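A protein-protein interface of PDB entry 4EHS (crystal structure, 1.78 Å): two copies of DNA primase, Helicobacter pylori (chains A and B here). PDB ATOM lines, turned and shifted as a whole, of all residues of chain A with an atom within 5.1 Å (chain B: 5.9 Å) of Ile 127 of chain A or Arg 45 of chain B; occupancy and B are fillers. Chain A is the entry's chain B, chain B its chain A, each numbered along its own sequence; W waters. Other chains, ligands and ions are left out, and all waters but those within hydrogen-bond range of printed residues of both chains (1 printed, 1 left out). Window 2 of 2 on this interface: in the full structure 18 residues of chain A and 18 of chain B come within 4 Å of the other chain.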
ATOM      1  N   SER A 123     -21.215 -15.737   7.866  1.00  0.00           N
ATOM      2  CA  SER A 123     -21.099 -16.846   8.765  1.00  0.00           C
ATOM      3  C   SER A 123     -20.609 -18.082   8.073  1.00  0.00           C
ATOM      4  O   SER A 123     -19.897 -18.867   8.669  1.00  0.00           O
ATOM      5  CB  SER A 123     -22.417 -17.150   9.497  1.00  0.00           C
ATOM      6  OG  SER A 123     -22.746 -16.032  10.305  1.00  0.00           O
ATOM      7  N   GLU A 124     -20.966 -18.246   6.813  1.00  0.00           N
ATOM      8  CA  GLU A 124     -20.522 -19.433   6.112  1.00  0.00           C
ATOM      9  C   GLU A 124     -19.028 -19.351   5.718  1.00  0.00           C
ATOM     10  O   GLU A 124     -18.317 -20.337   5.842  1.00  0.00           O
ATOM     11  CB  GLU A 124     -21.418 -19.671   4.906  1.00  0.00           C
ATOM     12  CG  GLU A 124     -22.886 -19.834   5.292  1.00  0.00           C
ATOM     13  CD  GLU A 124     -23.783 -19.808   4.041  1.00  0.00           C
ATOM     14  OE1 GLU A 124     -23.509 -20.596   3.146  1.00  0.00           O
ATOM     15  OE2 GLU A 124     -24.739 -18.989   3.950  1.00  0.00           O
ATOM     16  N   LYS A 125     -18.587 -18.171   5.307  1.00  0.00           N
ATOM     17  CA  LYS A 125     -17.150 -17.900   5.087  1.00  0.00           C
ATOM     18  C   LYS A 125     -16.410 -18.292   6.356  1.00  0.00           C
ATOM     19  O   LYS A 125     -15.393 -18.960   6.230  1.00  0.00           O
ATOM     20  CB  LYS A 125     -16.905 -16.442   4.744  1.00  0.00           C
ATOM     21  CG  LYS A 125     -17.334 -16.036   3.309  1.00  0.00           C
ATOM     22  CD  LYS A 125     -16.915 -14.577   3.060  1.00  0.00           C
ATOM     23  CE  LYS A 125     -17.191 -14.137   1.647  1.00  0.00           C
ATOM     24  NZ  LYS A 125     -18.473 -13.390   1.728  1.00  0.00           N
ATOM     25  N   MET A 126     -16.863 -17.848   7.550  1.00  0.00           N
ATOM     26  CA  MET A 126     -16.194 -18.204   8.795  1.00  0.00           C
ATOM     27  C   MET A 126     -16.058 -19.693   8.953  1.00  0.00           C
ATOM     28  O   MET A 126     -14.987 -20.154   9.291  1.00  0.00           O
ATOM     29  CB  MET A 126     -16.744 -17.627  10.097  1.00  0.00           C
ATOM     30  CG  MET A 126     -16.753 -16.090  10.027  1.00  0.00           C
ATOM     31  SD  MET A 126     -17.216 -15.460  11.842  1.00  0.00           S
ATOM     32  CE  MET A 126     -15.914 -16.481  12.859  1.00  0.00           C
ATOM     33  N   ILE A 127     -17.166 -20.432   8.774  1.00  0.00           N
ATOM     34  CA  ILE A 127     -17.129 -21.883   9.002  1.00  0.00           C
ATOM     35  C   ILE A 127     -16.156 -22.578   8.009  1.00  0.00           C
ATOM     36  O   ILE A 127     -15.330 -23.410   8.445  1.00  0.00           O
ATOM     37  CB  ILE A 127     -18.563 -22.482   8.938  1.00  0.00           C
ATOM     38  CG1 ILE A 127     -19.354 -21.978  10.112  1.00  0.00           C
ATOM     39  CG2 ILE A 127     -18.523 -23.977   8.938  1.00  0.00           C
ATOM     40  CD1 ILE A 127     -20.824 -22.422  10.086  1.00  0.00           C
ATOM     41  N   CYS A 128     -16.241 -22.192   6.751  1.00  0.00           N
ATOM     42  CA  CYS A 128     -15.395 -22.767   5.726  1.00  0.00           C
ATOM     43  C   CYS A 128     -13.928 -22.479   5.962  1.00  0.00           C
ATOM     44  O   CYS A 128     -13.136 -23.329   5.778  1.00  0.00           O
ATOM     45  CB  CYS A 128     -15.845 -22.363   4.324  1.00  0.00           C
ATOM     46  SG  CYS A 128     -17.517 -22.831   3.911  1.00  0.00           S
ATOM     47  N   LEU A 129     -13.592 -21.264   6.369  1.00  0.00           N
ATOM     48  CA  LEU A 129     -12.217 -20.914   6.606  1.00  0.00           C
ATOM     49  C   LEU A 129     -11.712 -21.620   7.837  1.00  0.00           C
ATOM     50  O   LEU A 129     -10.574 -21.970   7.911  1.00  0.00           O
ATOM     51  CB  LEU A 129     -12.065 -19.364   6.776  1.00  0.00           C
ATOM     52  CG  LEU A 129     -12.200 -18.593   5.459  1.00  0.00           C
ATOM     53  CD1 LEU A 129     -12.360 -17.073   5.820  1.00  0.00           C
ATOM     54  CD2 LEU A 129     -10.939 -18.696   4.621  1.00  0.00           C
ATOM     55  N   LYS A 130     -12.550 -21.792   8.845  1.00  0.00           N
ATOM     56  CA  LYS A 130     -12.064 -22.507  10.039  1.00  0.00           C
ATOM     57  C   LYS A 130     -11.794 -23.966   9.649  1.00  0.00           C
ATOM     58  O   LYS A 130     -10.832 -24.537  10.104  1.00  0.00           O
ATOM     59  CB  LYS A 130     -13.047 -22.371  11.217  1.00  0.00           C
ATOM     60  CG  LYS A 130     -12.733 -23.388  12.358  1.00  0.00           C
ATOM     61  CD  LYS A 130     -13.373 -23.132  13.739  1.00  0.00           C
ATOM     62  CE  LYS A 130     -14.751 -22.533  13.673  1.00  0.00           C
ATOM     63  NZ  LYS A 130     -15.010 -22.143  15.104  1.00  0.00           N
ATOM     64  N   LYS A 131     -12.685 -24.526   8.832  1.00  0.00           N
ATOM     65  CA  LYS A 131     -12.540 -25.909   8.329  1.00  0.00           C
ATOM     66  C   LYS A 131     -11.199 -25.983   7.586  1.00  0.00           C
ATOM     67  O   LYS A 131     -10.404 -26.928   7.786  1.00  0.00           O
ATOM     68  CB  LYS A 131     -13.721 -26.174   7.402  1.00  0.00           C
ATOM     69  CG  LYS A 131     -13.954 -27.573   6.846  1.00  0.00           C
ATOM     70  CD  LYS A 131     -15.299 -27.619   6.054  1.00  0.00           C
ATOM     71  CE  LYS A 131     -15.487 -28.936   5.258  1.00  0.00           C
ATOM     72  NZ  LYS A 131     -14.497 -29.106   4.127  1.00  0.00           N
ATOM     73  N   ALA A 132     -10.922 -24.994   6.724  1.00  0.00           N
ATOM     74  CA  ALA A 132      -9.633 -25.040   6.014  1.00  0.00           C
ATOM     75  C   ALA A 132      -8.414 -24.914   6.921  1.00  0.00           C
ATOM     76  O   ALA A 132      -7.416 -25.655   6.765  1.00  0.00           O
ATOM     77  CB  ALA A 132      -9.588 -23.993   4.870  1.00  0.00           C
ATOM     78  N   TYR B  40     -27.030 -31.642  19.510  1.00  0.00           N
ATOM     79  CA  TYR B  40     -25.657 -31.575  20.042  1.00  0.00           C
ATOM     80  C   TYR B  40     -24.917 -30.380  19.427  1.00  0.00           C
ATOM     81  O   TYR B  40     -24.220 -29.639  20.149  1.00  0.00           O
ATOM     82  CB  TYR B  40     -24.856 -32.792  19.682  1.00  0.00           C
ATOM     83  CG  TYR B  40     -24.962 -33.949  20.676  1.00  0.00           C
ATOM     84  CD1 TYR B  40     -24.274 -33.905  21.872  1.00  0.00           C
ATOM     85  CD2 TYR B  40     -25.749 -35.057  20.397  1.00  0.00           C
ATOM     86  CE1 TYR B  40     -24.330 -34.985  22.795  1.00  0.00           C
ATOM     87  CE2 TYR B  40     -25.826 -36.135  21.302  1.00  0.00           C
ATOM     88  CZ  TYR B  40     -25.141 -36.063  22.539  1.00  0.00           C
ATOM     89  OH  TYR B  40     -25.198 -37.113  23.433  1.00  0.00           O
ATOM     90  N   LEU B  41     -24.989 -30.231  18.100  1.00  0.00           N
ATOM     91  CA  LEU B  41     -24.337 -29.044  17.439  1.00  0.00           C
ATOM     92  C   LEU B  41     -24.899 -27.696  17.914  1.00  0.00           C
ATOM     93  O   LEU B  41     -24.147 -26.703  18.015  1.00  0.00           O
ATOM     94  CB  LEU B  41     -24.522 -29.117  15.921  1.00  0.00           C
ATOM     95  CG  LEU B  41     -24.179 -30.506  15.369  1.00  0.00           C
ATOM     96  CD1 LEU B  41     -24.385 -30.349  13.874  1.00  0.00           C
ATOM     97  CD2 LEU B  41     -22.747 -31.022  15.607  1.00  0.00           C
ATOM     98  N   LEU B  42     -26.184 -27.645  18.210  1.00  0.00           N
ATOM     99  CA  LEU B  42     -26.765 -26.408  18.750  1.00  0.00           C
ATOM    100  C   LEU B  42     -26.239 -26.097  20.158  1.00  0.00           C
ATOM    101  O   LEU B  42     -26.125 -24.894  20.549  1.00  0.00           O
ATOM    102  CB  LEU B  42     -28.304 -26.544  18.794  1.00  0.00           C
ATOM    103  CG  LEU B  42     -28.944 -26.335  17.413  1.00  0.00           C
ATOM    104  CD1 LEU B  42     -30.399 -26.877  17.543  1.00  0.00           C
ATOM    105  CD2 LEU B  42     -28.990 -24.847  16.978  1.00  0.00           C
ATOM    106  N   GLU B  43     -26.048 -27.128  20.961  1.00  0.00           N
ATOM    107  CA  GLU B  43     -25.649 -26.909  22.371  1.00  0.00           C
ATOM    108  C   GLU B  43     -24.156 -26.648  22.484  1.00  0.00           C
ATOM    109  O   GLU B  43     -23.701 -25.965  23.425  1.00  0.00           O
ATOM    110  CB  GLU B  43     -26.003 -28.087  23.266  1.00  0.00           C
ATOM    111  CG  GLU B  43     -27.537 -28.186  23.362  1.00  0.00           C
ATOM    112  CD  GLU B  43     -28.113 -28.366  24.764  1.00  0.00           C
ATOM    113  OE1 GLU B  43     -27.350 -28.470  25.747  1.00  0.00           O
ATOM    114  OE2 GLU B  43     -29.374 -28.579  24.852  1.00  0.00           O
ATOM    115  N   ASP B  44     -23.365 -27.204  21.536  1.00  0.00           N
ATOM    116  CA  ASP B  44     -21.920 -27.028  21.655  1.00  0.00           C
ATOM    117  C   ASP B  44     -21.357 -26.814  20.248  1.00  0.00           C
ATOM    118  O   ASP B  44     -21.191 -27.741  19.501  1.00  0.00           O
ATOM    119  CB  ASP B  44     -21.258 -28.183  22.409  1.00  0.00           C
ATOM    120  CG  ASP B  44     -19.738 -27.935  22.659  1.00  0.00           C
ATOM    121  OD1 ASP B  44     -19.127 -27.081  21.994  1.00  0.00           O
ATOM    122  OD2 ASP B  44     -19.231 -28.628  23.493  1.00  0.00           O
ATOM    123  N   ARG B  45     -21.118 -25.558  19.896  1.00  0.00           N
ATOM    124  CA  ARG B  45     -20.798 -25.250  18.478  1.00  0.00           C
ATOM    125  C   ARG B  45     -19.431 -25.816  18.149  1.00  0.00           C
ATOM    126  O   ARG B  45     -19.132 -25.994  16.950  1.00  0.00           O
ATOM    127  CB  ARG B  45     -20.876 -23.755  18.158  1.00  0.00           C
ATOM    128  CG  ARG B  45     -21.320 -23.472  16.697  1.00  0.00           C
ATOM    129  CD  ARG B  45     -21.775 -22.010  16.431  1.00  0.00           C
ATOM    130  NE  ARG B  45     -21.769 -21.638  15.012  1.00  0.00           N
ATOM    131  CZ  ARG B  45     -22.756 -21.892  14.125  1.00  0.00           C
ATOM    132  NH1 ARG B  45     -23.867 -22.530  14.488  1.00  0.00           N
ATOM    133  NH2 ARG B  45     -22.618 -21.531  12.846  1.00  0.00           N
ATOM    134  N   SER B  46     -18.608 -26.165  19.141  1.00  0.00           N
ATOM    135  CA  SER B  46     -17.261 -26.816  18.861  1.00  0.00           C
ATOM    136  C   SER B  46     -17.455 -28.187  18.226  1.00  0.00           C
ATOM    137  O   SER B  46     -16.644 -28.646  17.423  1.00  0.00           O
ATOM    138  CB  SER B  46     -16.402 -26.916  20.143  1.00  0.00           C
ATOM    139  OG  SER B  46     -16.859 -27.982  20.967  1.00  0.00           O
ATOM    140  N   LEU B  47     -18.599 -28.828  18.517  1.00  0.00           N
ATOM    141  CA  LEU B  47     -18.979 -30.074  17.840  1.00  0.00           C
ATOM    142  C   LEU B  47     -19.342 -29.878  16.352  1.00  0.00           C
ATOM    143  O   LEU B  47     -19.162 -30.828  15.565  1.00  0.00           O
ATOM    144  CB  LEU B  47     -20.162 -30.759  18.535  1.00  0.00           C
ATOM    145  CG  LEU B  47     -19.875 -31.015  20.004  1.00  0.00           C
ATOM    146  CD1 LEU B  47     -21.088 -31.677  20.676  1.00  0.00           C
ATOM    147  CD2 LEU B  47     -18.657 -31.891  20.247  1.00  0.00           C
ATOM    148  N   LEU B  48     -19.887 -28.710  15.978  1.00  0.00           N
ATOM    149  CA  LEU B  48     -20.132 -28.383  14.578  1.00  0.00           C
ATOM    150  C   LEU B  48     -18.764 -28.362  13.864  1.00  0.00           C
ATOM    151  O   LEU B  48     -18.628 -28.868  12.745  1.00  0.00           O
ATOM    152  CB  LEU B  48     -20.850 -27.036  14.448  1.00  0.00           C
ATOM    153  CG  LEU B  48     -21.135 -26.649  12.951  1.00  0.00           C
ATOM    154  CD1 LEU B  48     -22.068 -27.654  12.277  1.00  0.00           C
ATOM    155  CD2 LEU B  48     -21.807 -25.283  12.980  1.00  0.00           C
ATOM    156  N   ASP B  49     -17.744 -27.755  14.491  1.00  0.00           N
ATOM    157  CA  ASP B  49     -16.399 -27.726  13.876  1.00  0.00           C
ATOM    158  C   ASP B  49     -15.940 -29.134  13.491  1.00  0.00           C
ATOM    159  O   ASP B  49     -15.467 -29.365  12.381  1.00  0.00           O
ATOM    160  CB  ASP B  49     -15.372 -27.100  14.836  1.00  0.00           C
ATOM    161  CG  ASP B  49     -15.760 -25.666  15.294  1.00  0.00           C
ATOM    162  OD1 ASP B  49     -16.634 -24.983  14.716  1.00  0.00           O
ATOM    163  OD2 ASP B  49     -15.171 -25.248  16.323  1.00  0.00           O
ATOM    164  N   LEU B  50     -16.100 -30.091  14.414  1.00  0.00           N
ATOM    165  CA  LEU B  50     -15.749 -31.475  14.127  1.00  0.00           C
ATOM    166  C   LEU B  50     -16.641 -32.021  13.006  1.00  0.00           C
ATOM    167  O   LEU B  50     -16.166 -32.643  12.024  1.00  0.00           O
ATOM    168  CB  LEU B  50     -15.961 -32.323  15.392  1.00  0.00           C
ATOM    169  CG  LEU B  50     -15.674 -33.814  15.158  1.00  0.00           C
ATOM    170  CD1 LEU B  50     -14.223 -34.031  14.777  1.00  0.00           C
ATOM    171  CD2 LEU B  50     -16.024 -34.617  16.402  1.00  0.00           C
ATOM    172  N   VAL B  52     -18.367 -30.810  10.604  1.00  0.00           N
ATOM    173  CA  VAL B  52     -18.286 -30.381   9.189  1.00  0.00           C
ATOM    174  C   VAL B  52     -17.068 -31.014   8.455  1.00  0.00           C
ATOM    175  O   VAL B  52     -17.014 -30.912   7.234  1.00  0.00           O
ATOM    176  CB  VAL B  52     -18.331 -28.822   8.999  1.00  0.00           C
ATOM    177  CG1 VAL B  52     -19.646 -28.301   9.564  1.00  0.00           C
ATOM    178  CG2 VAL B  52     -17.131 -28.256   9.686  1.00  0.00           C
ATOM    179  N   LEU B  70     -28.388 -23.710  10.937  1.00  0.00           N
ATOM    180  CA  LEU B  70     -27.359 -23.736  11.971  1.00  0.00           C
ATOM    181  C   LEU B  70     -25.985 -23.417  11.392  1.00  0.00           C
ATOM    182  O   LEU B  70     -25.097 -22.945  12.102  1.00  0.00           O
ATOM    183  CB  LEU B  70     -27.333 -25.099  12.665  1.00  0.00           C
ATOM    184  CG  LEU B  70     -26.120 -25.384  13.552  1.00  0.00           C
ATOM    185  CD1 LEU B  70     -26.064 -24.408  14.717  1.00  0.00           C
ATOM    186  CD2 LEU B  70     -26.146 -26.821  14.053  1.00  0.00           C
ATOM    187  N   CYS B  71     -25.817 -23.676  10.100  1.00  0.00           N
ATOM    188  CA  CYS B  71     -24.558 -23.419   9.428  1.00  0.00           C
ATOM    189  C   CYS B  71     -24.437 -21.953   9.133  1.00  0.00           C
ATOM    190  O   CYS B  71     -23.317 -21.399   9.184  1.00  0.00           O
ATOM    191  CB  CYS B  71     -24.508 -24.205   8.124  1.00  0.00           C
ATOM    192  SG  CYS B  71     -24.077 -25.880   8.462  1.00  0.00           S
ATOM    193  N   GLN B  72     -25.558 -21.309   8.828  1.00  0.00           N
ATOM    194  CA  GLN B  72     -25.563 -19.883   8.521  1.00  0.00           C
ATOM    195  C   GLN B  72     -25.946 -19.055   9.743  1.00  0.00           C
ATOM    196  O   GLN B  72     -26.468 -17.948   9.616  1.00  0.00           O
ATOM    197  CB  GLN B  72     -26.520 -19.588   7.364  1.00  0.00           C
ATOM    198  CG  GLN B  72     -26.616 -20.704   6.337  1.00  0.00           C
ATOM    199  CD  GLN B  72     -27.863 -20.603   5.482  1.00  0.00           C
ATOM    200  OE1 GLN B  72     -28.313 -21.590   4.901  1.00  0.00           O
ATOM    201  NE2 GLN B  72     -28.430 -19.404   5.400  1.00  0.00           N
ATOM    202  N   GLU B  73     -25.685 -19.601  10.927  1.00  0.00           N
ATOM    203  CA  GLU B  73     -26.000 -18.917  12.166  1.00  0.00           C
ATOM    204  C   GLU B  73     -27.317 -18.188  12.114  1.00  0.00           C
ATOM    205  O   GLU B  73     -27.386 -17.055  12.599  1.00  0.00           O
ATOM    206  CB  GLU B  73     -24.901 -17.930  12.651  1.00  0.00           C
ATOM    207  CG  GLU B  73     -24.008 -18.505  13.688  1.00  0.00           C
ATOM    208  CD  GLU B  73     -22.770 -17.649  13.930  1.00  0.00           C
ATOM    209  OE1 GLU B  73     -22.339 -17.613  15.088  1.00  0.00           O
ATOM    210  OE2 GLU B  73     -22.254 -17.027  12.968  1.00  0.00           O
ATOM    211  N   LEU B  75     -29.714 -18.308  13.945  1.00  0.00           N
ATOM    212  CA  LEU B  75     -30.121 -18.872  15.225  1.00  0.00           C
ATOM    213  C   LEU B  75     -31.532 -18.479  15.714  1.00  0.00           C
ATOM    214  O   LEU B  75     -32.003 -18.996  16.737  1.00  0.00           O
ATOM    215  CB  LEU B  75     -29.026 -18.613  16.296  1.00  0.00           C
ATOM    216  CG  LEU B  75     -27.607 -19.112  15.900  1.00  0.00           C
ATOM    217  CD1 LEU B  75     -26.511 -18.868  16.957  1.00  0.00           C
ATOM    218  CD2 LEU B  75     -27.577 -20.574  15.488  1.00  0.00           C
HETATM  219  O   HOH W   1     -17.422 -22.990  16.323  1.00  0.00           O
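No position is printed for both chains. Of the 6 pairs that touch across the chains among the printed residues, none has its exchanged pair printed and touching as well.
OD1 of Asp 49 of chain B is in salt-bridge range of NZ of Lys 130 of chain A (3.3 Å). The side-chain carboxylate (OE2) of Glu 73 of chain B lies within hydrogen-bond range of the side-chain hydroxyl (OG) of Ser 123 of chain A, 2.9 Å away.
Among the printed residues, pairs that only touch across the chains: Glu 124 of chain A with Gln 72 of chain B (3.5 Å), Ile 127 of chain A with Arg 45 of chain B (3.4 Å), Ile 127 of chain A with Cys 71 of chain B (2.8 Å) and Lys 131 of chain A with Val 52 of chain B (3.2 Å).
Ile 127 of chain A touches just these residues of chain B: Arg 45 (3.4 Å) and Cys 71 (2.8 Å). Of the printed residues of chain A, Arg 45 of chain B touches Ile 127 (3.4 Å). Of the printed residues of chain A, Asp 49 of chain B touches Lys 130. Of the printed residues of chain B, Glu 124 of chain A touches Gln 72 (3.5 Å). Of the printed residues of chain A, Val 52 of chain B touches Lys 131 (3.2 Å). Cys 128 of chain A touches none of the printed residues of chain B. Leu 129 of chain A touches none of the printed residues of chain B. The nearest printed residue of chain B that does not touch Glu 124 of chain A is Cys 71 of chain B (4.2 Å).
The guanidinium group of Arg 45 of chain B lies within hydrogen-bond range of the backbone carbonyl oxygen of Leu 70 of chain B, at 2.7 Å.
Water W1 lies within hydrogen-bond range of the side-chain carboxylate of Asp 49 of chain B (2.7 Å) and the side-chain amino group of Lys 130 of chain A (2.8 Å).
Printed residues of chain A that touch a printed residue of chain B: Ser 123, Glu 124, Ile 127, Lys 130 and Lys 131. Among the printed residues, 6 pairs touch across the chains.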
